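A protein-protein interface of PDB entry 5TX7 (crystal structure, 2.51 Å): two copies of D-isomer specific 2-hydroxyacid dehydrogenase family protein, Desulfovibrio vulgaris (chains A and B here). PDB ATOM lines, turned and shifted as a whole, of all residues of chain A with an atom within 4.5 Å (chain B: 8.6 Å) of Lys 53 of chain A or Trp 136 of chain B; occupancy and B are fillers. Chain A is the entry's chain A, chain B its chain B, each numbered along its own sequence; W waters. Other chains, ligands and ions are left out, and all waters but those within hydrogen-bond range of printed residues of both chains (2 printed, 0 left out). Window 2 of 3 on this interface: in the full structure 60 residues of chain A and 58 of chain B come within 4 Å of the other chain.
Hydrophobic or aromatic side chains of chain A that line the printed part of chain B: His 286 and Trp 289.
Of the 10 printed residues of chain B, 5 touch a printed residue of chain A.
Hydrophobic or aromatic side chains of chain B that line the printed part of chain A: Trp 130, Trp 136 and Trp 139.
Among the printed residues, 12 pairs touch across the chains.
No position is printed for both chains.
Of the 12 pairs that touch across the chains among the printed residues, none has its exchanged pair printed and touching as well.
Among the printed residues, merely in contact across the chains: Thr 11 of chain A with Asp 135 of chain B (3.9 Å), Thr 11 of chain A with Trp 136 of chain B (3.9 Å), Thr 11 of chain A with Cys 137 of chain B (3.8 Å), Thr 11 of chain A with Trp 139 of chain B (3.2 Å), Asn 52 of chain A with Trp 136 of chain B (3.6 Å), Lys 53 of chain A with Trp 136 of chain B (3.6 Å), His 286 of chain A with Trp 130 of chain B (3.9 Å), His 286 of chain A with Trp 136 of chain B (3.9 Å), His 286 of chain A with Cys 137 of chain B (3.4 Å), Trp 289 of chain A with Trp 136 of chain B (3.4 Å), Trp 289 of chain A with Cys 137 of chain B (3.9 Å) and Trp 289 of chain A with Trp 139 of chain B (3.97 Å).
The side-chain carboxylate of Asp 8 of chain A lies within hydrogen-bond range of the backbone NH of Lys 53 of chain A (3.0 Å).
The side-chain amide oxygen of Asn 52 of chain A is in hydrogen-bond range of the side-chain amino group of Lys 53 of chain A, at 2.8 Å.
NE1 of Trp 289 of chain A is in hydrogen-bond range of O of His 286 of chain A (2.9 Å).
NE1 of Trp 130 of chain B sits at hydrogen-bond distance from O of Trp 136 of chain B, 2.8 Å away.
OG of Ser 133 of chain B sits at hydrogen-bond distance from O of Asp 135 of chain B (3.0 Å).
OG of Ser 133 of chain B sits at hydrogen-bond distance from O of Cys 137 of chain B.
Water W1 lies within hydrogen-bond range of the side-chain hydroxyl (OG1) of Thr 11 of chain A, the indole nitrogen (NE1) of Trp 136 of chain B and the side-chain carboxylate (OD2) of Asp 8 of chain A.
Water W2 lies within hydrogen-bond range of the side-chain carboxylate of Asp 135 of chain B (2.9 Å) and the backbone NH of Thr 11 of chain A (3.4 Å).
Lys 53 of chain A touches just one residue of chain B: Trp 136.
Trp 136 of chain B touches just these residues of chain A: Thr 11 (3.9 Å), Asn 52 (3.6 Å), Lys 53 (3.6 Å), His 286 (3.9 Å) and Trp 289 (3.4 Å).
Of the printed residues of chain B, Asn 52 of chain A touches Trp 136 (3.6 Å).
Of the printed residues of chain B, Trp 289 of chain A touches Trp 136, Cys 137 and Trp 139.
Of the printed residues of chain B, His 286 of chain A touches Trp 130 (3.9 Å), Trp 136 (3.9 Å) and Cys 137 (3.4 Å).
Printed residues of chain A within 4 Å of Trp 139 of chain B: Thr 11 (3.2 Å) and Trp 289 (3.97 Å).
Of the printed residues of chain A, Cys 137 of chain B touches Thr 11, His 286 and Trp 289.
Of the printed residues of chain A, Trp 130 of chain B touches His 286.
Pro 55 of chain A touches none of the printed residues of chain B.
Lys 79 of chain A touches none of the printed residues of chain B.
The nearest residue of chain B that does not touch Lys 53 of chain A is Cys 137 of chain B (7.3 Å).
The nearest printed residue of chain B that does not touch His 286 of chain A is Phe 138 of chain B (5.5 Å).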
ATOM      1  N   ASP A   8      26.128 -31.943  11.308  1.00  0.00           N
ATOM      2  CA  ASP A   8      25.527 -31.586  10.019  1.00  0.00           C
ATOM      3  C   ASP A   8      26.542 -30.970   9.084  1.00  0.00           C
ATOM      4  O   ASP A   8      26.549 -29.774   8.871  1.00  0.00           O
ATOM      5  CB  ASP A   8      24.288 -30.679  10.199  1.00  0.00           C
ATOM      6  CG  ASP A   8      24.589 -29.366  10.914  1.00  0.00           C
ATOM      7  OD1 ASP A   8      25.536 -29.318  11.731  1.00  0.00           O
ATOM      8  OD2 ASP A   8      23.847 -28.382  10.672  1.00  0.00           O
ATOM      9  N   THR A  11      26.092 -29.317   4.315  1.00  0.00           N
ATOM     10  CA  THR A  11      26.074 -27.926   3.835  1.00  0.00           C
ATOM     11  C   THR A  11      27.468 -27.253   3.847  1.00  0.00           C
ATOM     12  O   THR A  11      27.777 -26.486   2.938  1.00  0.00           O
ATOM     13  CB  THR A  11      25.075 -27.028   4.617  1.00  0.00           C
ATOM     14  OG1 THR A  11      25.366 -27.066   6.013  1.00  0.00           O
ATOM     15  CG2 THR A  11      23.617 -27.492   4.413  1.00  0.00           C
ATOM     16  N   THR A  51      28.779 -28.210  14.944  1.00  0.00           N
ATOM     17  CA  THR A  51      27.397 -28.004  14.565  1.00  0.00           C
ATOM     18  C   THR A  51      27.299 -26.716  13.750  1.00  0.00           C
ATOM     19  O   THR A  51      27.950 -25.729  14.056  1.00  0.00           O
ATOM     20  CB  THR A  51      26.459 -27.923  15.790  1.00  0.00           C
ATOM     21  OG1 THR A  51      25.121 -27.651  15.362  1.00  0.00           O
ATOM     22  CG2 THR A  51      26.877 -26.823  16.795  1.00  0.00           C
ATOM     23  N   ASN A  52      26.510 -26.754  12.687  1.00  0.00           N
ATOM     24  CA  ASN A  52      26.126 -25.557  11.965  1.00  0.00           C
ATOM     25  C   ASN A  52      24.783 -25.104  12.541  1.00  0.00           C
ATOM     26  O   ASN A  52      24.709 -24.088  13.208  1.00  0.00           O
ATOM     27  CB  ASN A  52      26.068 -25.834  10.452  1.00  0.00           C
ATOM     28  CG  ASN A  52      26.011 -24.567   9.619  1.00  0.00           C
ATOM     29  OD1 ASN A  52      25.555 -23.524  10.076  1.00  0.00           O
ATOM     30  ND2 ASN A  52      26.489 -24.661   8.380  1.00  0.00           N
ATOM     31  N   LYS A  53      23.736 -25.880  12.297  1.00  0.00           N
ATOM     32  CA  LYS A  53      22.387 -25.544  12.755  1.00  0.00           C
ATOM     33  C   LYS A  53      21.749 -26.629  13.622  1.00  0.00           C
ATOM     34  O   LYS A  53      20.570 -26.525  13.943  1.00  0.00           O
ATOM     35  CB  LYS A  53      21.473 -25.249  11.544  1.00  0.00           C
ATOM     36  CG  LYS A  53      21.890 -24.074  10.688  1.00  0.00           C
ATOM     37  CD  LYS A  53      21.846 -22.748  11.435  1.00  0.00           C
ATOM     38  CE  LYS A  53      22.265 -21.581  10.536  1.00  0.00           C
ATOM     39  NZ  LYS A  53      23.746 -21.400  10.488  1.00  0.00           N
ATOM     40  N   VAL A  54      22.496 -27.664  14.002  1.00  0.00           N
ATOM     41  CA  VAL A  54      21.959 -28.681  14.912  1.00  0.00           C
ATOM     42  C   VAL A  54      21.905 -28.070  16.317  1.00  0.00           C
ATOM     43  O   VAL A  54      22.907 -27.551  16.800  1.00  0.00           O
ATOM     44  CB  VAL A  54      22.792 -29.964  14.907  1.00  0.00           C
ATOM     45  CG1 VAL A  54      22.282 -30.940  15.965  1.00  0.00           C
ATOM     46  CG2 VAL A  54      22.724 -30.611  13.524  1.00  0.00           C
ATOM     47  N   PRO A  55      20.728 -28.096  16.950  1.00  0.00           N
ATOM     48  CA  PRO A  55      20.587 -27.426  18.244  1.00  0.00           C
ATOM     49  C   PRO A  55      21.221 -28.194  19.397  1.00  0.00           C
ATOM     50  O   PRO A  55      21.179 -29.413  19.387  1.00  0.00           O
ATOM     51  CB  PRO A  55      19.063 -27.315  18.427  1.00  0.00           C
ATOM     52  CG  PRO A  55      18.502 -28.391  17.571  1.00  0.00           C
ATOM     53  CD  PRO A  55      19.439 -28.586  16.432  1.00  0.00           C
ATOM     54  N   ALA A  74      29.615 -21.428  11.657  1.00  0.00           N
ATOM     55  CA  ALA A  74      28.827 -20.251  11.343  1.00  0.00           C
ATOM     56  C   ALA A  74      29.320 -19.110  12.221  1.00  0.00           C
ATOM     57  O   ALA A  74      30.095 -19.319  13.140  1.00  0.00           O
ATOM     58  CB  ALA A  74      27.337 -20.510  11.611  1.00  0.00           C
ATOM     59  N   LYS A  79      21.071 -21.339  17.952  1.00  0.00           N
ATOM     60  CA  LYS A  79      20.534 -22.659  18.324  1.00  0.00           C
ATOM     61  C   LYS A  79      21.399 -23.425  19.358  1.00  0.00           C
ATOM     62  O   LYS A  79      21.065 -24.538  19.727  1.00  0.00           O
ATOM     63  CB  LYS A  79      20.283 -23.500  17.060  1.00  0.00           C
ATOM     64  CG  LYS A  79      19.190 -22.909  16.159  1.00  0.00           C
ATOM     65  CD  LYS A  79      18.998 -23.643  14.831  1.00  0.00           C
ATOM     66  CE  LYS A  79      17.900 -24.709  14.890  1.00  0.00           C
ATOM     67  NZ  LYS A  79      17.931 -25.680  13.743  1.00  0.00           N
ATOM     68  N   HIS A 286      18.731 -19.017   1.323  1.00  0.00           N
ATOM     69  CA  HIS A 286      19.694 -18.823   2.396  1.00  0.00           C
ATOM     70  C   HIS A 286      21.070 -19.393   2.059  1.00  0.00           C
ATOM     71  O   HIS A 286      21.625 -20.187   2.811  1.00  0.00           O
ATOM     72  CB  HIS A 286      19.134 -19.419   3.686  1.00  0.00           C
ATOM     73  CG  HIS A 286      19.734 -18.851   4.928  1.00  0.00           C
ATOM     74  ND1 HIS A 286      19.150 -19.014   6.169  1.00  0.00           N
ATOM     75  CD2 HIS A 286      20.866 -18.135   5.131  1.00  0.00           C
ATOM     76  CE1 HIS A 286      19.906 -18.429   7.085  1.00  0.00           C
ATOM     77  NE2 HIS A 286      20.942 -17.873   6.479  1.00  0.00           N
ATOM     78  N   TRP A 289      25.988 -16.909   2.088  1.00  0.00           N
ATOM     79  CA  TRP A 289      27.212 -17.323   2.817  1.00  0.00           C
ATOM     80  C   TRP A 289      28.051 -18.412   2.179  1.00  0.00           C
ATOM     81  O   TRP A 289      29.156 -18.698   2.660  1.00  0.00           O
ATOM     82  CB  TRP A 289      26.814 -17.858   4.209  1.00  0.00           C
ATOM     83  CG  TRP A 289      26.005 -19.145   4.112  1.00  0.00           C
ATOM     84  CD1 TRP A 289      24.666 -19.253   3.864  1.00  0.00           C
ATOM     85  CD2 TRP A 289      26.504 -20.492   4.208  1.00  0.00           C
ATOM     86  NE1 TRP A 289      24.302 -20.578   3.812  1.00  0.00           N
ATOM     87  CE2 TRP A 289      25.408 -21.358   4.014  1.00  0.00           C
ATOM     88  CE3 TRP A 289      27.770 -21.046   4.450  1.00  0.00           C
ATOM     89  CZ2 TRP A 289      25.528 -22.750   4.069  1.00  0.00           C
ATOM     90  CZ3 TRP A 289      27.897 -22.435   4.486  1.00  0.00           C
ATOM     91  CH2 TRP A 289      26.779 -23.277   4.290  1.00  0.00           C
ATOM     92  N   ALA B 129      11.251 -26.552  -3.858  1.00  0.00           N
ATOM     93  CA  ALA B 129      12.530 -27.232  -3.610  1.00  0.00           C
ATOM     94  C   ALA B 129      13.101 -26.978  -2.206  1.00  0.00           C
ATOM     95  O   ALA B 129      13.849 -27.818  -1.680  1.00  0.00           O
ATOM     96  CB  ALA B 129      13.553 -26.859  -4.672  1.00  0.00           C
ATOM     97  N   TRP B 130      12.738 -25.845  -1.610  1.00  0.00           N
ATOM     98  CA  TRP B 130      13.186 -25.496  -0.260  1.00  0.00           C
ATOM     99  C   TRP B 130      12.488 -26.371   0.794  1.00  0.00           C
ATOM    100  O   TRP B 130      13.142 -26.857   1.721  1.00  0.00           O
ATOM    101  CB  TRP B 130      12.976 -23.986   0.029  1.00  0.00           C
ATOM    102  CG  TRP B 130      13.921 -23.377   1.054  1.00  0.00           C
ATOM    103  CD1 TRP B 130      14.728 -24.045   1.940  1.00  0.00           C
ATOM    104  CD2 TRP B 130      14.121 -21.978   1.317  1.00  0.00           C
ATOM    105  NE1 TRP B 130      15.416 -23.157   2.716  1.00  0.00           N
ATOM    106  CE2 TRP B 130      15.066 -21.881   2.363  1.00  0.00           C
ATOM    107  CE3 TRP B 130      13.601 -20.797   0.761  1.00  0.00           C
ATOM    108  CZ2 TRP B 130      15.509 -20.655   2.867  1.00  0.00           C
ATOM    109  CZ3 TRP B 130      14.029 -19.573   1.274  1.00  0.00           C
ATOM    110  CH2 TRP B 130      14.982 -19.517   2.320  1.00  0.00           C
ATOM    111  N   THR B 131      11.175 -26.579   0.641  1.00  0.00           N
ATOM    112  CA  THR B 131      10.417 -27.542   1.485  1.00  0.00           C
ATOM    113  C   THR B 131      10.908 -28.980   1.298  1.00  0.00           C
ATOM    114  O   THR B 131      11.056 -29.718   2.278  1.00  0.00           O
ATOM    115  CB  THR B 131       8.890 -27.549   1.179  1.00  0.00           C
ATOM    116  OG1 THR B 131       8.369 -26.226   1.187  1.00  0.00           O
ATOM    117  CG2 THR B 131       8.143 -28.352   2.215  1.00  0.00           C
ATOM    118  N   SER B 133      13.837 -29.911   0.360  1.00  0.00           N
ATOM    119  CA  SER B 133      15.231 -30.038   0.782  1.00  0.00           C
ATOM    120  C   SER B 133      15.353 -30.664   2.170  1.00  0.00           C
ATOM    121  O   SER B 133      14.612 -30.298   3.079  1.00  0.00           O
ATOM    122  CB  SER B 133      15.939 -28.670   0.768  1.00  0.00           C
ATOM    123  OG  SER B 133      17.283 -28.755   1.215  1.00  0.00           O
ATOM    124  N   PRO B 134      16.294 -31.613   2.334  1.00  0.00           N
ATOM    125  CA  PRO B 134      16.551 -32.169   3.666  1.00  0.00           C
ATOM    126  C   PRO B 134      17.342 -31.224   4.588  1.00  0.00           C
ATOM    127  O   PRO B 134      17.445 -31.507   5.779  1.00  0.00           O
ATOM    128  CB  PRO B 134      17.361 -33.446   3.360  1.00  0.00           C
ATOM    129  CG  PRO B 134      18.084 -33.134   2.082  1.00  0.00           C
ATOM    130  CD  PRO B 134      17.183 -32.208   1.305  1.00  0.00           C
ATOM    131  N   ASP B 135      17.896 -30.134   4.051  1.00  0.00           N
ATOM    132  CA  ASP B 135      18.618 -29.123   4.842  1.00  0.00           C
ATOM    133  C   ASP B 135      17.931 -27.756   4.829  1.00  0.00           C
ATOM    134  O   ASP B 135      17.235 -27.414   3.880  1.00  0.00           O
ATOM    135  CB  ASP B 135      20.039 -28.945   4.305  1.00  0.00           C
ATOM    136  CG  ASP B 135      20.833 -30.210   4.324  1.00  0.00           C
ATOM    137  OD1 ASP B 135      21.050 -30.793   5.413  1.00  0.00           O
ATOM    138  OD2 ASP B 135      21.239 -30.645   3.240  1.00  0.00           O
ATOM    139  N   TRP B 136      18.158 -26.987   5.892  1.00  0.00           N
ATOM    140  CA  TRP B 136      17.771 -25.549   6.029  1.00  0.00           C
ATOM    141  C   TRP B 136      18.061 -24.620   4.827  1.00  0.00           C
ATOM    142  O   TRP B 136      17.409 -23.595   4.646  1.00  0.00           O
ATOM    143  CB  TRP B 136      18.417 -24.953   7.304  1.00  0.00           C
ATOM    144  CG  TRP B 136      19.940 -25.003   7.320  1.00  0.00           C
ATOM    145  CD1 TRP B 136      20.718 -26.069   7.674  1.00  0.00           C
ATOM    146  CD2 TRP B 136      20.842 -23.946   6.985  1.00  0.00           C
ATOM    147  NE1 TRP B 136      22.040 -25.755   7.547  1.00  0.00           N
ATOM    148  CE2 TRP B 136      22.155 -24.455   7.143  1.00  0.00           C
ATOM    149  CE3 TRP B 136      20.676 -22.617   6.577  1.00  0.00           C
ATOM    150  CZ2 TRP B 136      23.304 -23.682   6.916  1.00  0.00           C
ATOM    151  CZ3 TRP B 136      21.838 -21.834   6.344  1.00  0.00           C
ATOM    152  CH2 TRP B 136      23.128 -22.378   6.514  1.00  0.00           C
ATOM    153  N   CYS B 137      19.054 -24.965   4.035  1.00  0.00           N
ATOM    154  CA  CYS B 137      19.340 -24.294   2.779  1.00  0.00           C
ATOM    155  C   CYS B 137      19.660 -25.335   1.721  1.00  0.00           C
ATOM    156  O   CYS B 137      19.758 -26.522   2.021  1.00  0.00           O
ATOM    157  CB  CYS B 137      20.538 -23.368   2.947  1.00  0.00           C
ATOM    158  SG  CYS B 137      22.040 -24.249   3.367  1.00  0.00           S
ATOM    159  N   PHE B 138      19.822 -24.884   0.481  1.00  0.00           N
ATOM    160  CA  PHE B 138      20.287 -25.755  -0.598  1.00  0.00           C
ATOM    161  C   PHE B 138      20.862 -24.939  -1.756  1.00  0.00           C
ATOM    162  O   PHE B 138      20.700 -23.728  -1.814  1.00  0.00           O
ATOM    163  CB  PHE B 138      19.151 -26.664  -1.096  1.00  0.00           C
ATOM    164  CG  PHE B 138      18.142 -25.955  -1.960  1.00  0.00           C
ATOM    165  CD1 PHE B 138      17.095 -25.280  -1.386  1.00  0.00           C
ATOM    166  CD2 PHE B 138      18.255 -25.962  -3.341  1.00  0.00           C
ATOM    167  CE1 PHE B 138      16.171 -24.613  -2.167  1.00  0.00           C
ATOM    168  CE2 PHE B 138      17.333 -25.315  -4.131  1.00  0.00           C
ATOM    169  CZ  PHE B 138      16.281 -24.640  -3.541  1.00  0.00           C
ATOM    170  N   TRP B 139      21.494 -25.634  -2.692  1.00  0.00           N
ATOM    171  CA  TRP B 139      21.922 -25.084  -3.949  1.00  0.00           C
ATOM    172  C   TRP B 139      22.044 -26.217  -4.980  1.00  0.00           C
ATOM    173  O   TRP B 139      22.625 -27.265  -4.692  1.00  0.00           O
ATOM    174  CB  TRP B 139      23.213 -24.251  -3.834  1.00  0.00           C
ATOM    175  CG  TRP B 139      24.415 -24.928  -3.222  1.00  0.00           C
ATOM    176  CD1 TRP B 139      25.361 -25.696  -3.861  1.00  0.00           C
ATOM    177  CD2 TRP B 139      24.809 -24.870  -1.849  1.00  0.00           C
ATOM    178  NE1 TRP B 139      26.311 -26.133  -2.950  1.00  0.00           N
ATOM    179  CE2 TRP B 139      26.000 -25.629  -1.715  1.00  0.00           C
ATOM    180  CE3 TRP B 139      24.274 -24.245  -0.720  1.00  0.00           C
ATOM    181  CZ2 TRP B 139      26.663 -25.771  -0.500  1.00  0.00           C
ATOM    182  CZ3 TRP B 139      24.933 -24.398   0.501  1.00  0.00           C
ATOM    183  CH2 TRP B 139      26.113 -25.154   0.597  1.00  0.00           C
HETATM  184  O   HOH W   1      23.598 -28.046   7.882  1.00  0.00           O
HETATM  185  O   HOH W   2      23.684 -30.309   6.553  1.00  0.00           O
